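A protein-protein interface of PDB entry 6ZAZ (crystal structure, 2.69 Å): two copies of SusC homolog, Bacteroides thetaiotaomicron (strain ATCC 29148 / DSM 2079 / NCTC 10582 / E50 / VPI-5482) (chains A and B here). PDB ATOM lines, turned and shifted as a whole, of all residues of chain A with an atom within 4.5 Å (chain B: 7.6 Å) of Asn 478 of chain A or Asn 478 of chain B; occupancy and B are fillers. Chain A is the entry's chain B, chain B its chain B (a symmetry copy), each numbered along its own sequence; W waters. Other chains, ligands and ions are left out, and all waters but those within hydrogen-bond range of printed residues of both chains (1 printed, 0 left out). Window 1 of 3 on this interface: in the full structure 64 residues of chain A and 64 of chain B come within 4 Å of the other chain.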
ATOM      1  N   THR A 448       4.571 -37.805 -24.521  1.00  0.00           N
ATOM      2  CA  THR A 448       4.967 -37.425 -25.871  1.00  0.00           C
ATOM      3  C   THR A 448       6.420 -36.971 -25.823  1.00  0.00           C
ATOM      4  O   THR A 448       6.774 -36.083 -25.036  1.00  0.00           O
ATOM      5  CB  THR A 448       4.071 -36.307 -26.423  1.00  0.00           C
ATOM      6  OG1 THR A 448       2.707 -36.739 -26.392  1.00  0.00           O
ATOM      7  CG2 THR A 448       4.460 -35.922 -27.851  1.00  0.00           C
ATOM      8  N   TYR A 449       7.247 -37.561 -26.680  1.00  0.00           N
ATOM      9  CA  TYR A 449       8.695 -37.482 -26.570  1.00  0.00           C
ATOM     10  C   TYR A 449       9.261 -37.074 -27.920  1.00  0.00           C
ATOM     11  O   TYR A 449       9.139 -37.818 -28.897  1.00  0.00           O
ATOM     12  CB  TYR A 449       9.240 -38.836 -26.109  1.00  0.00           C
ATOM     13  CG  TYR A 449      10.736 -38.984 -25.954  1.00  0.00           C
ATOM     14  CD1 TYR A 449      11.516 -39.457 -26.996  1.00  0.00           C
ATOM     15  CD2 TYR A 449      11.356 -38.718 -24.748  1.00  0.00           C
ATOM     16  CE1 TYR A 449      12.870 -39.630 -26.849  1.00  0.00           C
ATOM     17  CE2 TYR A 449      12.725 -38.891 -24.589  1.00  0.00           C
ATOM     18  CZ  TYR A 449      13.477 -39.349 -25.643  1.00  0.00           C
ATOM     19  OH  TYR A 449      14.844 -39.523 -25.506  1.00  0.00           O
ATOM     20  N   TRP A 450       9.879 -35.897 -27.973  1.00  0.00           N
ATOM     21  CA  TRP A 450      10.524 -35.380 -29.172  1.00  0.00           C
ATOM     22  C   TRP A 450      12.045 -35.404 -28.979  1.00  0.00           C
ATOM     23  O   TRP A 450      12.576 -34.751 -28.070  1.00  0.00           O
ATOM     24  CB  TRP A 450      10.055 -33.958 -29.453  1.00  0.00           C
ATOM     25  CG  TRP A 450       8.669 -33.724 -30.032  1.00  0.00           C
ATOM     26  CD1 TRP A 450       7.525 -33.460 -29.331  1.00  0.00           C
ATOM     27  CD2 TRP A 450       8.314 -33.606 -31.427  1.00  0.00           C
ATOM     28  NE1 TRP A 450       6.479 -33.215 -30.194  1.00  0.00           N
ATOM     29  CE2 TRP A 450       6.933 -33.296 -31.484  1.00  0.00           C
ATOM     30  CE3 TRP A 450       9.024 -33.743 -32.628  1.00  0.00           C
ATOM     31  CZ2 TRP A 450       6.250 -33.119 -32.696  1.00  0.00           C
ATOM     32  CZ3 TRP A 450       8.340 -33.580 -33.838  1.00  0.00           C
ATOM     33  CH2 TRP A 450       6.964 -33.273 -33.857  1.00  0.00           C
ATOM     34  N   TYR A 476      19.157 -33.883 -28.114  1.00  0.00           N
ATOM     35  CA  TYR A 476      18.203 -33.102 -27.324  1.00  0.00           C
ATOM     36  C   TYR A 476      16.840 -33.756 -27.410  1.00  0.00           C
ATOM     37  O   TYR A 476      16.274 -33.870 -28.507  1.00  0.00           O
ATOM     38  CB  TYR A 476      18.090 -31.653 -27.810  1.00  0.00           C
ATOM     39  CG  TYR A 476      16.932 -30.921 -27.174  1.00  0.00           C
ATOM     40  CD1 TYR A 476      16.715 -30.988 -25.811  1.00  0.00           C
ATOM     41  CD2 TYR A 476      16.052 -30.167 -27.932  1.00  0.00           C
ATOM     42  CE1 TYR A 476      15.657 -30.333 -25.224  1.00  0.00           C
ATOM     43  CE2 TYR A 476      14.986 -29.509 -27.353  1.00  0.00           C
ATOM     44  CZ  TYR A 476      14.801 -29.591 -25.997  1.00  0.00           C
ATOM     45  OH  TYR A 476      13.753 -28.955 -25.384  1.00  0.00           O
ATOM     46  N   ALA A 477      16.315 -34.164 -26.253  1.00  0.00           N
ATOM     47  CA  ALA A 477      14.973 -34.717 -26.140  1.00  0.00           C
ATOM     48  C   ALA A 477      14.179 -33.939 -25.102  1.00  0.00           C
ATOM     49  O   ALA A 477      14.748 -33.354 -24.171  1.00  0.00           O
ATOM     50  CB  ALA A 477      14.989 -36.196 -25.752  1.00  0.00           C
ATOM     51  N   ASN A 478      12.858 -33.927 -25.274  1.00  0.00           N
ATOM     52  CA  ASN A 478      11.960 -33.360 -24.278  1.00  0.00           C
ATOM     53  C   ASN A 478      10.733 -34.260 -24.167  1.00  0.00           C
ATOM     54  O   ASN A 478      10.227 -34.775 -25.171  1.00  0.00           O
ATOM     55  CB  ASN A 478      11.588 -31.885 -24.615  1.00  0.00           C
ATOM     56  CG  ASN A 478      10.279 -31.759 -25.375  1.00  0.00           C
ATOM     57  OD1 ASN A 478       9.201 -31.877 -24.791  1.00  0.00           O
ATOM     58  ND2 ASN A 478      10.365 -31.515 -26.683  1.00  0.00           N
ATOM     59  N   LYS A 479      10.272 -34.473 -22.936  1.00  0.00           N
ATOM     60  CA  LYS A 479       9.188 -35.404 -22.681  1.00  0.00           C
ATOM     61  C   LYS A 479       8.119 -34.684 -21.889  1.00  0.00           C
ATOM     62  O   LYS A 479       8.419 -34.066 -20.863  1.00  0.00           O
ATOM     63  CB  LYS A 479       9.687 -36.626 -21.919  1.00  0.00           C
ATOM     64  CG  LYS A 479       8.671 -37.702 -21.778  1.00  0.00           C
ATOM     65  CD  LYS A 479       9.056 -38.659 -20.683  1.00  0.00           C
ATOM     66  CE  LYS A 479       9.502 -39.996 -21.231  1.00  0.00           C
ATOM     67  NZ  LYS A 479       9.035 -41.096 -20.323  1.00  0.00           N
ATOM     68  N   GLN A 480       6.893 -34.732 -22.396  1.00  0.00           N
ATOM     69  CA  GLN A 480       5.712 -34.120 -21.799  1.00  0.00           C
ATOM     70  C   GLN A 480       4.726 -35.234 -21.488  1.00  0.00           C
ATOM     71  O   GLN A 480       4.697 -36.250 -22.190  1.00  0.00           O
ATOM     72  CB  GLN A 480       5.081 -33.071 -22.759  1.00  0.00           C
ATOM     73  CG  GLN A 480       3.651 -32.668 -22.424  1.00  0.00           C
ATOM     74  CD  GLN A 480       2.736 -32.848 -23.627  1.00  0.00           C
ATOM     75  OE1 GLN A 480       2.891 -32.146 -24.644  1.00  0.00           O
ATOM     76  NE2 GLN A 480       1.773 -33.793 -23.520  1.00  0.00           N
ATOM     77  N   GLN A 505       7.126 -32.281 -17.219  1.00  0.00           N
ATOM     78  CA  GLN A 505       7.980 -31.878 -18.319  1.00  0.00           C
ATOM     79  C   GLN A 505       9.402 -32.241 -17.956  1.00  0.00           C
ATOM     80  O   GLN A 505       9.790 -32.145 -16.790  1.00  0.00           O
ATOM     81  CB  GLN A 505       7.899 -30.363 -18.597  1.00  0.00           C
ATOM     82  CG  GLN A 505       8.732 -29.901 -19.792  1.00  0.00           C
ATOM     83  CD  GLN A 505       8.228 -30.452 -21.103  1.00  0.00           C
ATOM     84  OE1 GLN A 505       7.028 -30.621 -21.291  1.00  0.00           O
ATOM     85  NE2 GLN A 505       9.139 -30.717 -22.027  1.00  0.00           N
ATOM     86  N   GLU A 506      10.172 -32.665 -18.958  1.00  0.00           N
ATOM     87  CA  GLU A 506      11.582 -32.973 -18.772  1.00  0.00           C
ATOM     88  C   GLU A 506      12.302 -32.651 -20.060  1.00  0.00           C
ATOM     89  O   GLU A 506      11.776 -32.896 -21.144  1.00  0.00           O
ATOM     90  CB  GLU A 506      11.844 -34.445 -18.433  1.00  0.00           C
ATOM     91  CG  GLU A 506      10.742 -35.149 -17.653  1.00  0.00           C
ATOM     92  CD  GLU A 506      11.084 -36.585 -17.320  1.00  0.00           C
ATOM     93  OE1 GLU A 506      10.358 -37.472 -17.807  1.00  0.00           O
ATOM     94  OE2 GLU A 506      12.056 -36.835 -16.576  1.00  0.00           O
ATOM     95  N   HIS A 507      13.510 -32.130 -19.917  1.00  0.00           N
ATOM     96  CA  HIS A 507      14.416 -31.855 -21.014  1.00  0.00           C
ATOM     97  C   HIS A 507      15.759 -32.511 -20.724  1.00  0.00           C
ATOM     98  O   HIS A 507      16.250 -32.480 -19.587  1.00  0.00           O
ATOM     99  CB  HIS A 507      14.628 -30.345 -21.207  1.00  0.00           C
ATOM    100  CG  HIS A 507      13.374 -29.562 -21.417  1.00  0.00           C
ATOM    101  ND1 HIS A 507      12.935 -29.193 -22.671  1.00  0.00           N
ATOM    102  CD2 HIS A 507      12.488 -29.038 -20.532  1.00  0.00           C
ATOM    103  CE1 HIS A 507      11.834 -28.469 -22.545  1.00  0.00           C
ATOM    104  NE2 HIS A 507      11.544 -28.358 -21.259  1.00  0.00           N
ATOM    105  N   ASN B 391      15.704 -24.414 -34.963  1.00  0.00           N
ATOM    106  CA  ASN B 391      16.134 -23.184 -34.316  1.00  0.00           C
ATOM    107  C   ASN B 391      15.995 -23.274 -32.804  1.00  0.00           C
ATOM    108  O   ASN B 391      15.004 -23.805 -32.288  1.00  0.00           O
ATOM    109  CB  ASN B 391      15.312 -21.987 -34.811  1.00  0.00           C
ATOM    110  CG  ASN B 391      15.488 -21.740 -36.291  1.00  0.00           C
ATOM    111  OD1 ASN B 391      14.722 -22.252 -37.075  1.00  0.00           O
ATOM    112  ND2 ASN B 391      16.468 -20.939 -36.673  1.00  0.00           N
ATOM    113  N   THR B 393      16.297 -20.405 -29.765  1.00  0.00           N
ATOM    114  CA  THR B 393      16.464 -19.033 -29.304  1.00  0.00           C
ATOM    115  C   THR B 393      16.312 -18.998 -27.801  1.00  0.00           C
ATOM    116  O   THR B 393      15.761 -19.925 -27.198  1.00  0.00           O
ATOM    117  CB  THR B 393      15.437 -18.066 -29.891  1.00  0.00           C
ATOM    118  OG1 THR B 393      14.247 -18.116 -29.089  1.00  0.00           O
ATOM    119  CG2 THR B 393      15.110 -18.394 -31.332  1.00  0.00           C
ATOM    120  N   TYR B 447      14.103 -17.454 -20.967  1.00  0.00           N
ATOM    121  CA  TYR B 447      13.373 -18.548 -21.593  1.00  0.00           C
ATOM    122  C   TYR B 447      14.245 -19.160 -22.684  1.00  0.00           C
ATOM    123  O   TYR B 447      15.098 -18.483 -23.265  1.00  0.00           O
ATOM    124  CB  TYR B 447      12.016 -18.098 -22.166  1.00  0.00           C
ATOM    125  CG  TYR B 447      12.080 -17.234 -23.434  1.00  0.00           C
ATOM    126  CD1 TYR B 447      12.359 -17.793 -24.679  1.00  0.00           C
ATOM    127  CD2 TYR B 447      11.837 -15.874 -23.381  1.00  0.00           C
ATOM    128  CE1 TYR B 447      12.425 -17.018 -25.820  1.00  0.00           C
ATOM    129  CE2 TYR B 447      11.880 -15.093 -24.525  1.00  0.00           C
ATOM    130  CZ  TYR B 447      12.176 -15.671 -25.742  1.00  0.00           C
ATOM    131  OH  TYR B 447      12.229 -14.877 -26.869  1.00  0.00           O
ATOM    132  N   THR B 448      14.021 -20.449 -22.949  1.00  0.00           N
ATOM    133  CA  THR B 448      14.691 -21.190 -24.009  1.00  0.00           C
ATOM    134  C   THR B 448      13.622 -21.775 -24.921  1.00  0.00           C
ATOM    135  O   THR B 448      12.713 -22.474 -24.454  1.00  0.00           O
ATOM    136  CB  THR B 448      15.578 -22.305 -23.436  1.00  0.00           C
ATOM    137  OG1 THR B 448      16.527 -21.733 -22.532  1.00  0.00           O
ATOM    138  CG2 THR B 448      16.309 -23.071 -24.539  1.00  0.00           C
ATOM    139  N   TYR B 449      13.748 -21.508 -26.217  1.00  0.00           N
ATOM    140  CA  TYR B 449      12.676 -21.715 -27.180  1.00  0.00           C
ATOM    141  C   TYR B 449      13.229 -22.504 -28.356  1.00  0.00           C
ATOM    142  O   TYR B 449      14.103 -22.016 -29.077  1.00  0.00           O
ATOM    143  CB  TYR B 449      12.120 -20.359 -27.614  1.00  0.00           C
ATOM    144  CG  TYR B 449      11.008 -20.341 -28.639  1.00  0.00           C
ATOM    145  CD1 TYR B 449      11.288 -20.227 -29.990  1.00  0.00           C
ATOM    146  CD2 TYR B 449       9.683 -20.367 -28.250  1.00  0.00           C
ATOM    147  CE1 TYR B 449      10.282 -20.173 -30.922  1.00  0.00           C
ATOM    148  CE2 TYR B 449       8.658 -20.311 -29.186  1.00  0.00           C
ATOM    149  CZ  TYR B 449       8.963 -20.211 -30.521  1.00  0.00           C
ATOM    150  OH  TYR B 449       7.956 -20.160 -31.469  1.00  0.00           O
ATOM    151  N   TRP B 450      12.720 -23.718 -28.547  1.00  0.00           N
ATOM    152  CA  TRP B 450      13.096 -24.582 -29.658  1.00  0.00           C
ATOM    153  C   TRP B 450      11.927 -24.678 -30.645  1.00  0.00           C
ATOM    154  O   TRP B 450      10.836 -25.141 -30.287  1.00  0.00           O
ATOM    155  CB  TRP B 450      13.463 -25.969 -29.146  1.00  0.00           C
ATOM    156  CG  TRP B 450      14.799 -26.187 -28.452  1.00  0.00           C
ATOM    157  CD1 TRP B 450      15.036 -26.142 -27.107  1.00  0.00           C
ATOM    158  CD2 TRP B 450      16.040 -26.605 -29.060  1.00  0.00           C
ATOM    159  NE1 TRP B 450      16.347 -26.478 -26.839  1.00  0.00           N
ATOM    160  CE2 TRP B 450      16.985 -26.767 -28.016  1.00  0.00           C
ATOM    161  CE3 TRP B 450      16.446 -26.847 -30.380  1.00  0.00           C
ATOM    162  CZ2 TRP B 450      18.310 -27.163 -28.253  1.00  0.00           C
ATOM    163  CZ3 TRP B 450      17.772 -27.229 -30.618  1.00  0.00           C
ATOM    164  CH2 TRP B 450      18.685 -27.378 -29.555  1.00  0.00           C
ATOM    165  N   ARG B 451      12.151 -24.271 -31.888  1.00  0.00           N
ATOM    166  CA  ARG B 451      11.118 -24.348 -32.913  1.00  0.00           C
ATOM    167  C   ARG B 451      11.602 -25.218 -34.067  1.00  0.00           C
ATOM    168  O   ARG B 451      12.712 -25.031 -34.575  1.00  0.00           O
ATOM    169  CB  ARG B 451      10.729 -22.949 -33.416  1.00  0.00           C
ATOM    170  CG  ARG B 451       9.773 -22.945 -34.629  1.00  0.00           C
ATOM    171  CD  ARG B 451       9.154 -21.591 -34.813  1.00  0.00           C
ATOM    172  NE  ARG B 451       8.409 -21.460 -36.065  1.00  0.00           N
ATOM    173  CZ  ARG B 451       8.137 -20.289 -36.650  1.00  0.00           C
ATOM    174  NH1 ARG B 451       8.575 -19.159 -36.098  1.00  0.00           N
ATOM    175  NH2 ARG B 451       7.449 -20.238 -37.793  1.00  0.00           N
ATOM    176  N   MET B 452      10.770 -26.162 -34.485  1.00  0.00           N
ATOM    177  CA  MET B 452      11.070 -26.993 -35.639  1.00  0.00           C
ATOM    178  C   MET B 452      10.058 -26.678 -36.721  1.00  0.00           C
ATOM    179  O   MET B 452       8.849 -26.746 -36.481  1.00  0.00           O
ATOM    180  CB  MET B 452      11.025 -28.466 -35.276  1.00  0.00           C
ATOM    181  CG  MET B 452      12.146 -28.831 -34.368  1.00  0.00           C
ATOM    182  SD  MET B 452      12.018 -30.542 -33.885  1.00  0.00           S
ATOM    183  CE  MET B 452      10.263 -30.681 -33.644  1.00  0.00           C
ATOM    184  N   TYR B 476       6.308 -26.706 -34.883  1.00  0.00           N
ATOM    185  CA  TYR B 476       6.296 -27.159 -33.490  1.00  0.00           C
ATOM    186  C   TYR B 476       7.355 -26.402 -32.716  1.00  0.00           C
ATOM    187  O   TYR B 476       8.548 -26.501 -33.037  1.00  0.00           O
ATOM    188  CB  TYR B 476       6.568 -28.662 -33.361  1.00  0.00           C
ATOM    189  CG  TYR B 476       6.811 -29.083 -31.931  1.00  0.00           C
ATOM    190  CD1 TYR B 476       5.975 -28.658 -30.916  1.00  0.00           C
ATOM    191  CD2 TYR B 476       7.876 -29.900 -31.592  1.00  0.00           C
ATOM    192  CE1 TYR B 476       6.194 -29.028 -29.610  1.00  0.00           C
ATOM    193  CE2 TYR B 476       8.106 -30.274 -30.283  1.00  0.00           C
ATOM    194  CZ  TYR B 476       7.255 -29.839 -29.301  1.00  0.00           C
ATOM    195  OH  TYR B 476       7.451 -30.186 -27.989  1.00  0.00           O
ATOM    196  N   ALA B 477       6.914 -25.665 -31.693  1.00  0.00           N
ATOM    197  CA  ALA B 477       7.804 -24.959 -30.782  1.00  0.00           C
ATOM    198  C   ALA B 477       7.502 -25.364 -29.348  1.00  0.00           C
ATOM    199  O   ALA B 477       6.376 -25.760 -29.020  1.00  0.00           O
ATOM    200  CB  ALA B 477       7.672 -23.440 -30.910  1.00  0.00           C
ATOM    201  N   ASN B 478       8.522 -25.273 -28.496  1.00  0.00           N
ATOM    202  CA  ASN B 478       8.346 -25.476 -27.065  1.00  0.00           C
ATOM    203  C   ASN B 478       9.195 -24.447 -26.324  1.00  0.00           C
ATOM    204  O   ASN B 478      10.324 -24.144 -26.728  1.00  0.00           O
ATOM    205  CB  ASN B 478       8.681 -26.938 -26.646  1.00  0.00           C
ATOM    206  CG  ASN B 478      10.108 -27.105 -26.151  1.00  0.00           C
ATOM    207  OD1 ASN B 478      10.428 -26.728 -25.023  1.00  0.00           O
ATOM    208  ND2 ASN B 478      10.973 -27.671 -26.993  1.00  0.00           N
ATOM    209  N   LYS B 479       8.637 -23.888 -25.253  1.00  0.00           N
ATOM    210  CA  LYS B 479       9.289 -22.810 -24.531  1.00  0.00           C
ATOM    211  C   LYS B 479       9.361 -23.191 -23.069  1.00  0.00           C
ATOM    212  O   LYS B 479       8.343 -23.566 -22.477  1.00  0.00           O
ATOM    213  CB  LYS B 479       8.530 -21.500 -24.707  1.00  0.00           C
ATOM    214  CG  LYS B 479       9.235 -20.318 -24.144  1.00  0.00           C
ATOM    215  CD  LYS B 479       8.283 -19.168 -23.958  1.00  0.00           C
ATOM    216  CE  LYS B 479       8.524 -18.064 -24.963  1.00  0.00           C
ATOM    217  NZ  LYS B 479       8.302 -16.731 -24.313  1.00  0.00           N
ATOM    218  N   GLN B 480      10.566 -23.136 -22.515  1.00  0.00           N
ATOM    219  CA  GLN B 480      10.866 -23.449 -21.123  1.00  0.00           C
ATOM    220  C   GLN B 480      11.430 -22.191 -20.483  1.00  0.00           C
ATOM    221  O   GLN B 480      12.071 -21.383 -21.163  1.00  0.00           O
ATOM    222  CB  GLN B 480      11.876 -24.626 -21.022  1.00  0.00           C
ATOM    223  CG  GLN B 480      12.559 -24.776 -19.668  1.00  0.00           C
ATOM    224  CD  GLN B 480      14.073 -24.800 -19.819  1.00  0.00           C
ATOM    225  OE1 GLN B 480      14.631 -25.743 -20.410  1.00  0.00           O
ATOM    226  NE2 GLN B 480      14.753 -23.758 -19.284  1.00  0.00           N
ATOM    227  N   ALA B 481      11.139 -21.999 -19.193  1.00  0.00           N
ATOM    228  CA  ALA B 481      11.683 -20.889 -18.421  1.00  0.00           C
ATOM    229  C   ALA B 481      11.417 -21.130 -16.944  1.00  0.00           C
ATOM    230  O   ALA B 481      10.316 -21.542 -16.571  1.00  0.00           O
ATOM    231  CB  ALA B 481      11.063 -19.534 -18.826  1.00  0.00           C
ATOM    232  N   LYS B 504       8.044 -22.979 -15.918  1.00  0.00           N
ATOM    233  CA  LYS B 504       6.978 -22.841 -16.900  1.00  0.00           C
ATOM    234  C   LYS B 504       7.354 -23.576 -18.172  1.00  0.00           C
ATOM    235  O   LYS B 504       8.496 -23.498 -18.631  1.00  0.00           O
ATOM    236  CB  LYS B 504       6.709 -21.368 -17.258  1.00  0.00           C
ATOM    237  CG  LYS B 504       6.009 -20.541 -16.196  1.00  0.00           C
ATOM    238  CD  LYS B 504       5.501 -19.192 -16.753  1.00  0.00           C
ATOM    239  CE  LYS B 504       4.297 -19.340 -17.693  1.00  0.00           C
ATOM    240  NZ  LYS B 504       3.656 -18.022 -17.941  1.00  0.00           N
ATOM    241  N   GLN B 505       6.378 -24.242 -18.760  1.00  0.00           N
ATOM    242  CA  GLN B 505       6.554 -24.996 -19.986  1.00  0.00           C
ATOM    243  C   GLN B 505       5.365 -24.713 -20.876  1.00  0.00           C
ATOM    244  O   GLN B 505       4.245 -24.560 -20.386  1.00  0.00           O
ATOM    245  CB  GLN B 505       6.645 -26.514 -19.732  1.00  0.00           C
ATOM    246  CG  GLN B 505       6.897 -27.346 -20.988  1.00  0.00           C
ATOM    247  CD  GLN B 505       8.252 -27.084 -21.599  1.00  0.00           C
ATOM    248  OE1 GLN B 505       9.221 -26.835 -20.890  1.00  0.00           O
ATOM    249  NE2 GLN B 505       8.335 -27.156 -22.918  1.00  0.00           N
ATOM    250  N   GLU B 506       5.618 -24.635 -22.182  1.00  0.00           N
ATOM    251  CA  GLU B 506       4.559 -24.447 -23.164  1.00  0.00           C
ATOM    252  C   GLU B 506       4.971 -25.154 -24.433  1.00  0.00           C
ATOM    253  O   GLU B 506       6.144 -25.129 -24.806  1.00  0.00           O
ATOM    254  CB  GLU B 506       4.297 -22.975 -23.500  1.00  0.00           C
ATOM    255  CG  GLU B 506       4.555 -21.984 -22.373  1.00  0.00           C
ATOM    256  CD  GLU B 506       4.236 -20.557 -22.763  1.00  0.00           C
ATOM    257  OE1 GLU B 506       5.180 -19.743 -22.767  1.00  0.00           O
ATOM    258  OE2 GLU B 506       3.065 -20.238 -23.054  1.00  0.00           O
ATOM    259  N   HIS B 507       3.992 -25.753 -25.091  1.00  0.00           N
ATOM    260  CA  HIS B 507       4.144 -26.388 -26.384  1.00  0.00           C
ATOM    261  C   HIS B 507       3.093 -25.831 -27.336  1.00  0.00           C
ATOM    262  O   HIS B 507       1.931 -25.634 -26.956  1.00  0.00           O
ATOM    263  CB  HIS B 507       3.975 -27.911 -26.289  1.00  0.00           C
ATOM    264  CG  HIS B 507       4.893 -28.581 -25.319  1.00  0.00           C
ATOM    265  ND1 HIS B 507       6.061 -29.197 -25.713  1.00  0.00           N
ATOM    266  CD2 HIS B 507       4.794 -28.770 -23.978  1.00  0.00           C
ATOM    267  CE1 HIS B 507       6.638 -29.743 -24.654  1.00  0.00           C
ATOM    268  NE2 HIS B 507       5.887 -29.501 -23.591  1.00  0.00           N
ATOM    269  N   TRP B 508       3.525 -25.572 -28.565  1.00  0.00           N
ATOM    270  CA  TRP B 508       2.652 -25.248 -29.681  1.00  0.00           C
ATOM    271  C   TRP B 508       2.988 -26.212 -30.806  1.00  0.00           C
ATOM    272  O   TRP B 508       4.117 -26.194 -31.319  1.00  0.00           O
ATOM    273  CB  TRP B 508       2.855 -23.808 -30.161  1.00  0.00           C
ATOM    274  CG  TRP B 508       2.650 -22.723 -29.144  1.00  0.00           C
ATOM    275  CD1 TRP B 508       1.502 -22.040 -28.914  1.00  0.00           C
ATOM    276  CD2 TRP B 508       3.635 -22.165 -28.263  1.00  0.00           C
ATOM    277  NE1 TRP B 508       1.691 -21.108 -27.929  1.00  0.00           N
ATOM    278  CE2 TRP B 508       2.994 -21.158 -27.511  1.00  0.00           C
ATOM    279  CE3 TRP B 508       4.995 -22.429 -28.026  1.00  0.00           C
ATOM    280  CZ2 TRP B 508       3.662 -20.399 -26.541  1.00  0.00           C
ATOM    281  CZ3 TRP B 508       5.660 -21.680 -27.065  1.00  0.00           C
ATOM    282  CH2 TRP B 508       4.988 -20.673 -26.333  1.00  0.00           C
ATOM    283  N   THR B 509       2.012 -27.031 -31.205  1.00  0.00           N
ATOM    284  CA  THR B 509       2.214 -28.044 -32.241  1.00  0.00           C
ATOM    285  C   THR B 509       1.211 -27.838 -33.375  1.00  0.00           C
ATOM    286  O   THR B 509       0.029 -28.181 -33.242  1.00  0.00           O
ATOM    287  CB  THR B 509       2.075 -29.445 -31.644  1.00  0.00           C
ATOM    288  OG1 THR B 509       2.948 -29.564 -30.526  1.00  0.00           O
ATOM    289  CG2 THR B 509       2.473 -30.472 -32.646  1.00  0.00           C
HETATM  290  O   HOH W   1       4.254 -31.851 -29.194  1.00  0.00           O
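OH of Tyr 476 of chain A sits at hydrogen-bond distance from ND2 of Asn 478 of chain B (3.5 Å).
The side-chain amide nitrogen (ND2) of Asn 478 of chain A lies within hydrogen-bond range of the side-chain hydroxyl (OH) of Tyr 476 of chain B.
NE2 of His 507 of chain B lies within hydrogen-bond range of OE1 of Gln 505 of chain A, 2.8 Å away.
The side-chain amide oxygen (OE1) of Gln 505 of chain B is in hydrogen-bond range of a ring nitrogen (NE2) of His 507 of chain A, at 2.8 Å.
Asn 478 of chain A touches just these residues of chain B: Tyr 476, Asn 478 and His 507.
Printed residues of chain A within 4 Å of Trp 450 of chain B: Tyr 476.
Of the printed residues of chain B, Tyr 476 of chain A touches Trp 450 (3.4 Å) and Asn 478 (3.5 Å).
Of the printed residues of chain B, Trp 450 of chain A touches Met 452 and Tyr 476.
Printed residues of chain B within 4 Å of Gln 505 of chain A: Gln 505 and His 507.
Arg 451 of chain B touches none of the printed residues of chain A.
Ala 477 of chain A touches none of the printed residues of chain B.
The nearest printed residue of chain A that does not touch Asn 478 of chain B is Gln 505 of chain A (5.2 Å).
The nearest printed residue of chain B that does not touch Tyr 476 of chain A is Gln 480 of chain B (6.0 Å).
The backbone carbonyl oxygen of Gln 480 of chain A lies within hydrogen-bond range of the backbone NH of Thr 448 of chain A (2.8 Å).
O of Trp 450 of chain A is in hydrogen-bond range of N of Asn 478 of chain A (2.9 Å).
A ring nitrogen (ND1) of His 507 of chain A sits at hydrogen-bond distance from the side-chain hydroxyl (OH) of Tyr 476 of chain A, at 2.8 Å.
The backbone NH of Thr 448 of chain B sits at hydrogen-bond distance from the backbone carbonyl oxygen of Gln 480 of chain B (2.8 Å).
The backbone carbonyl oxygen (O) of Tyr 476 of chain B sits at hydrogen-bond distance from the backbone NH (N) of Met 452 of chain B (2.7 Å).
A ring nitrogen (NE2) of His 507 of chain B sits at hydrogen-bond distance from the side-chain amide nitrogen of Gln 505 of chain B (3.5 Å).
Of the 11 printed residues of chain A, 6 touch a printed residue of chain B.
Printed residues of chain A that touch a printed residue of chain B: Trp 450, Tyr 476, Asn 478, Gln 480, Gln 505 and His 507.
Along chain A the printed residues that touch a printed residue of chain B span positions 450 to 507.
Of the 20 printed residues of chain B, 7 touch a printed residue of chain A.
Printed residues of chain B that touch a printed residue of chain A: Trp 450, Met 452, Tyr 476, Asn 478, Gln 480, Gln 505 and His 507.
Hydrophobic or aromatic side chains of chain B that line the printed part of chain A: Trp 450, Met 452, Tyr 476 and His 507.
Among the printed residues, no Asp or Glu carboxylate lies within 4 Å of a Lys or Arg side-chain nitrogen of the other chain.
Trp 450 of chain A touches Met 452 of chain B.
Trp 450 of chain A touches Tyr 476 of chain B.
NE1 of Trp 450 of chain B touches CE2 of Tyr 476 of chain A, 3.4 Å away.
ND2 of Asn 478 of chain A touches ND2 of Asn 478 of chain B (3.9 Å).
Asn 478 of chain A touches His 507 of chain B (OD1 to CE1, 3.3 Å).
NE2 of His 507 of chain B touches CB of Gln 480 of chain A (3.8 Å).
Gln 505 of chain B touches Gln 505 of chain A.
His 507 of chain A touches Asn 478 of chain B (CE1 to OD1, 3.3 Å).
Gln 480 of chain B touches His 507 of chain A (CB to NE2, 3.8 Å).
Trp 450 of chain A touches Tyr 476 of chain B, and with the chains exchanged Tyr 476 of chain A touches Trp 450 of chain B.
Asn 478 of chain A touches His 507 of chain B, and with the chains exchanged His 507 of chain A touches Asn 478 of chain B.
Gln 480 of chain A touches His 507 of chain B, and with the chains exchanged His 507 of chain A touches Gln 480 of chain B.
Gln 505 of chain A touches His 507 of chain B, and with the chains exchanged His 507 of chain A touches Gln 505 of chain B.
Of the 13 pairs that touch across the chains among the printed residues, 12 have their exchanged pair printed and touching as well.
Water W1 lies within hydrogen-bond range of the indole nitrogen (NE1) of Trp 450 of chain A and the side-chain hydroxyl (OG1) of Thr 509 of chain B.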
